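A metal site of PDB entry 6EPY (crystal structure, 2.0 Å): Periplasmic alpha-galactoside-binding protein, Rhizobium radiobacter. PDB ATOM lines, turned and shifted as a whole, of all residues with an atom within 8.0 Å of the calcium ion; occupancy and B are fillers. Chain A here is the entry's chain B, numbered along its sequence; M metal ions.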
ATOM      1  N   LYS A 457      19.701  23.364  -9.964  1.00  0.00           N
ATOM      2  CA  LYS A 457      18.656  24.266  -9.476  1.00  0.00           C
ATOM      3  C   LYS A 457      19.135  25.148  -8.325  1.00  0.00           C
ATOM      4  O   LYS A 457      20.026  24.750  -7.559  1.00  0.00           O
ATOM      5  CB  LYS A 457      17.351  23.522  -9.124  1.00  0.00           C
ATOM      6  CG  LYS A 457      17.334  22.684  -7.846  1.00  0.00           C
ATOM      7  CD  LYS A 457      15.974  21.982  -7.624  1.00  0.00           C
ATOM      8  CE  LYS A 457      14.884  22.748  -6.869  1.00  0.00           C
ATOM      9  NZ  LYS A 457      14.723  22.301  -5.469  1.00  0.00           N
ATOM     10  N   ASP A 458      18.566  26.340  -8.215  1.00  0.00           N
ATOM     11  CA  ASP A 458      18.912  27.282  -7.160  1.00  0.00           C
ATOM     12  C   ASP A 458      18.245  26.807  -5.862  1.00  0.00           C
ATOM     13  O   ASP A 458      17.017  26.775  -5.779  1.00  0.00           O
ATOM     14  CB  ASP A 458      18.476  28.703  -7.538  1.00  0.00           C
ATOM     15  CG  ASP A 458      18.801  29.790  -6.533  1.00  0.00           C
ATOM     16  OD1 ASP A 458      19.732  29.599  -5.727  1.00  0.00           O
ATOM     17  OD2 ASP A 458      18.146  30.846  -6.591  1.00  0.00           O
ATOM     18  N   THR A 459      19.070  26.367  -4.892  1.00  0.00           N
ATOM     19  CA  THR A 459      18.606  25.824  -3.603  1.00  0.00           C
ATOM     20  C   THR A 459      18.822  26.790  -2.426  1.00  0.00           C
ATOM     21  O   THR A 459      18.498  26.441  -1.295  1.00  0.00           O
ATOM     22  CB  THR A 459      19.226  24.439  -3.355  1.00  0.00           C
ATOM     23  OG1 THR A 459      20.653  24.544  -3.358  1.00  0.00           O
ATOM     24  CG2 THR A 459      18.791  23.388  -4.380  1.00  0.00           C
ATOM     25  N   ASP A 460      19.356  28.006  -2.689  1.00  0.00           N
ATOM     26  CA  ASP A 460      19.612  28.990  -1.626  1.00  0.00           C
ATOM     27  C   ASP A 460      19.029  30.405  -1.945  1.00  0.00           C
ATOM     28  O   ASP A 460      19.340  31.382  -1.251  1.00  0.00           O
ATOM     29  CB  ASP A 460      21.123  29.051  -1.276  1.00  0.00           C
ATOM     30  CG  ASP A 460      22.086  29.130  -2.442  1.00  0.00           C
ATOM     31  OD1 ASP A 460      21.787  29.866  -3.413  1.00  0.00           O
ATOM     32  OD2 ASP A 460      23.162  28.505  -2.379  1.00  0.00           O
ATOM     33  N   GLY A 461      18.168  30.465  -2.968  1.00  0.00           N
ATOM     34  CA  GLY A 461      17.488  31.682  -3.418  1.00  0.00           C
ATOM     35  C   GLY A 461      18.325  32.858  -3.905  1.00  0.00           C
ATOM     36  O   GLY A 461      17.809  33.973  -3.982  1.00  0.00           O
ATOM     37  N   ASP A 462      19.600  32.642  -4.266  1.00  0.00           N
ATOM     38  CA  ASP A 462      20.429  33.756  -4.729  1.00  0.00           C
ATOM     39  C   ASP A 462      20.387  33.973  -6.270  1.00  0.00           C
ATOM     40  O   ASP A 462      21.141  34.783  -6.794  1.00  0.00           O
ATOM     41  CB  ASP A 462      21.889  33.633  -4.215  1.00  0.00           C
ATOM     42  CG  ASP A 462      22.764  32.539  -4.806  1.00  0.00           C
ATOM     43  OD1 ASP A 462      22.237  31.693  -5.573  1.00  0.00           O
ATOM     44  OD2 ASP A 462      23.958  32.497  -4.467  1.00  0.00           O
ATOM     45  N   GLY A 463      19.515  33.247  -6.963  1.00  0.00           N
ATOM     46  CA  GLY A 463      19.376  33.369  -8.418  1.00  0.00           C
ATOM     47  C   GLY A 463      20.376  32.567  -9.237  1.00  0.00           C
ATOM     48  O   GLY A 463      20.258  32.490 -10.461  1.00  0.00           O
ATOM     49  N   PHE A 464      21.372  31.951  -8.568  1.00  0.00           N
ATOM     50  CA  PHE A 464      22.389  31.129  -9.210  1.00  0.00           C
ATOM     51  C   PHE A 464      22.171  29.652  -8.934  1.00  0.00           C
ATOM     52  O   PHE A 464      21.858  29.267  -7.806  1.00  0.00           O
ATOM     53  CB  PHE A 464      23.797  31.569  -8.805  1.00  0.00           C
ATOM     54  CG  PHE A 464      24.172  32.911  -9.397  1.00  0.00           C
ATOM     55  CD1 PHE A 464      24.494  33.030 -10.740  1.00  0.00           C
ATOM     56  CD2 PHE A 464      24.175  34.059  -8.612  1.00  0.00           C
ATOM     57  CE1 PHE A 464      24.854  34.258 -11.293  1.00  0.00           C
ATOM     58  CE2 PHE A 464      24.520  35.299  -9.171  1.00  0.00           C
ATOM     59  CZ  PHE A 464      24.879  35.386 -10.501  1.00  0.00           C
ATOM     60  N   LEU A 465      22.324  28.834  -9.982  1.00  0.00           N
ATOM     61  CA  LEU A 465      22.114  27.404  -9.884  1.00  0.00           C
ATOM     62  C   LEU A 465      23.176  26.705  -9.059  1.00  0.00           C
ATOM     63  O   LEU A 465      24.373  27.029  -9.158  1.00  0.00           O
ATOM     64  CB  LEU A 465      21.999  26.767 -11.282  1.00  0.00           C
ATOM     65  CG  LEU A 465      20.919  27.343 -12.203  1.00  0.00           C
ATOM     66  CD1 LEU A 465      21.185  26.983 -13.623  1.00  0.00           C
ATOM     67  CD2 LEU A 465      19.537  26.885 -11.785  1.00  0.00           C
ATOM     68  N   ASN A 466      22.718  25.781  -8.216  1.00  0.00           N
ATOM     69  CA  ASN A 466      23.536  24.963  -7.335  1.00  0.00           C
ATOM     70  C   ASN A 466      23.698  23.582  -7.917  1.00  0.00           C
ATOM     71  O   ASN A 466      22.786  23.079  -8.610  1.00  0.00           O
ATOM     72  CB  ASN A 466      22.855  24.820  -5.960  1.00  0.00           C
ATOM     73  CG  ASN A 466      22.800  26.088  -5.184  1.00  0.00           C
ATOM     74  OD1 ASN A 466      22.027  27.002  -5.486  1.00  0.00           O
ATOM     75  ND2 ASN A 466      23.586  26.162  -4.124  1.00  0.00           N
ATOM     76  N   PHE A 467      24.818  22.925  -7.586  1.00  0.00           N
ATOM     77  CA  PHE A 467      25.033  21.539  -7.937  1.00  0.00           C
ATOM     78  C   PHE A 467      24.062  20.706  -7.079  1.00  0.00           C
ATOM     79  O   PHE A 467      23.679  21.178  -5.989  1.00  0.00           O
ATOM     80  CB  PHE A 467      26.456  21.104  -7.539  1.00  0.00           C
ATOM     81  CG  PHE A 467      27.542  21.544  -8.484  1.00  0.00           C
ATOM     82  CD1 PHE A 467      27.720  20.905  -9.711  1.00  0.00           C
ATOM     83  CD2 PHE A 467      28.433  22.538  -8.124  1.00  0.00           C
ATOM     84  CE1 PHE A 467      28.751  21.300 -10.568  1.00  0.00           C
ATOM     85  CE2 PHE A 467      29.467  22.932  -8.994  1.00  0.00           C
ATOM     86  CZ  PHE A 467      29.627  22.295 -10.204  1.00  0.00           C
ATOM     87  N   GLY A 474      26.521  20.626  -2.669  1.00  0.00           N
ATOM     88  CA  GLY A 474      25.382  21.379  -3.180  1.00  0.00           C
ATOM     89  C   GLY A 474      25.597  22.865  -3.346  1.00  0.00           C
ATOM     90  O   GLY A 474      24.625  23.626  -3.413  1.00  0.00           O
ATOM     91  N   ARG A 475      26.868  23.316  -3.420  1.00  0.00           N
ATOM     92  CA  ARG A 475      27.208  24.729  -3.581  1.00  0.00           C
ATOM     93  C   ARG A 475      26.852  25.256  -4.981  1.00  0.00           C
ATOM     94  O   ARG A 475      26.575  24.458  -5.881  1.00  0.00           O
ATOM     95  CB  ARG A 475      28.715  24.986  -3.286  1.00  0.00           C
ATOM     96  CG  ARG A 475      29.630  24.548  -4.413  1.00  0.00           C
ATOM     97  CD  ARG A 475      31.076  24.817  -4.070  1.00  0.00           C
ATOM     98  NE  ARG A 475      31.575  23.804  -3.144  1.00  0.00           N
ATOM     99  CZ  ARG A 475      32.837  23.432  -3.028  1.00  0.00           C
ATOM    100  NH1 ARG A 475      33.778  24.021  -3.773  1.00  0.00           N
ATOM    101  NH2 ARG A 475      33.183  22.475  -2.189  1.00  0.00           N
ATOM    102  N   ASN A 476      26.891  26.582  -5.157  1.00  0.00           N
ATOM    103  CA  ASN A 476      26.665  27.212  -6.441  1.00  0.00           C
ATOM    104  C   ASN A 476      27.679  26.752  -7.477  1.00  0.00           C
ATOM    105  O   ASN A 476      28.866  26.582  -7.157  1.00  0.00           O
ATOM    106  CB  ASN A 476      26.747  28.731  -6.338  1.00  0.00           C
ATOM    107  CG  ASN A 476      25.496  29.412  -5.843  1.00  0.00           C
ATOM    108  OD1 ASN A 476      24.384  28.902  -5.976  1.00  0.00           O
ATOM    109  ND2 ASN A 476      25.675  30.609  -5.325  1.00  0.00           N
ATOM    110  N   VAL A 477      27.205  26.539  -8.716  1.00  0.00           N
ATOM    111  CA  VAL A 477      28.060  26.240  -9.839  1.00  0.00           C
ATOM    112  C   VAL A 477      28.868  27.545 -10.081  1.00  0.00           C
ATOM    113  O   VAL A 477      28.283  28.637 -10.134  1.00  0.00           O
ATOM    114  CB  VAL A 477      27.239  25.850 -11.103  1.00  0.00           C
ATOM    115  CG1 VAL A 477      28.150  25.637 -12.331  1.00  0.00           C
ATOM    116  CG2 VAL A 477      26.375  24.613 -10.844  1.00  0.00           C
ATOM    117  N   GLY A 505      21.248  31.603 -15.033  1.00  0.00           N
ATOM    118  CA  GLY A 505      21.484  31.182 -13.652  1.00  0.00           C
ATOM    119  C   GLY A 505      22.864  30.608 -13.394  1.00  0.00           C
ATOM    120  O   GLY A 505      23.101  30.065 -12.318  1.00  0.00           O
HETATM  121 CA    CA M   1      22.091  29.445  -5.603  1.00  0.00          CA
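OD2 of Asp 458 lies within hydrogen-bond range of N of Gly 463.
The side-chain carboxylate of Asp 458 lies close to the backbone NH of Gly 461, at 3.3 Å.
The side-chain amide nitrogen (ND2) of Asn 466 lies close to the side-chain hydroxyl (OG1) of Thr 459 (3.4 Å).
The backbone NH (N) of Asn 466 lies within hydrogen-bond range of the backbone carbonyl oxygen (O) of Lys 457 (3.0 Å).
ND2 of Asn 466 is in hydrogen-bond range of O of Gly 474 (2.8 Å).
The calcium ion is bound by the backbone carbonyl oxygen (O) of Phe 464 (2.2 Å), the side-chain carboxylate (OD1) of Asp 460 (2.3 Å), the side-chain carboxylate (OD1) of Asp 462 (2.3 Å), the side-chain carboxylate (OD1) of Asp 458 (2.4 Å), the side-chain amide oxygen (OD1) of Asn 476 (2.4 Å) and the side-chain amide oxygen (OD1) of Asn 466 (2.4 Å).
The calcium ion has six donor atoms within binding distance.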
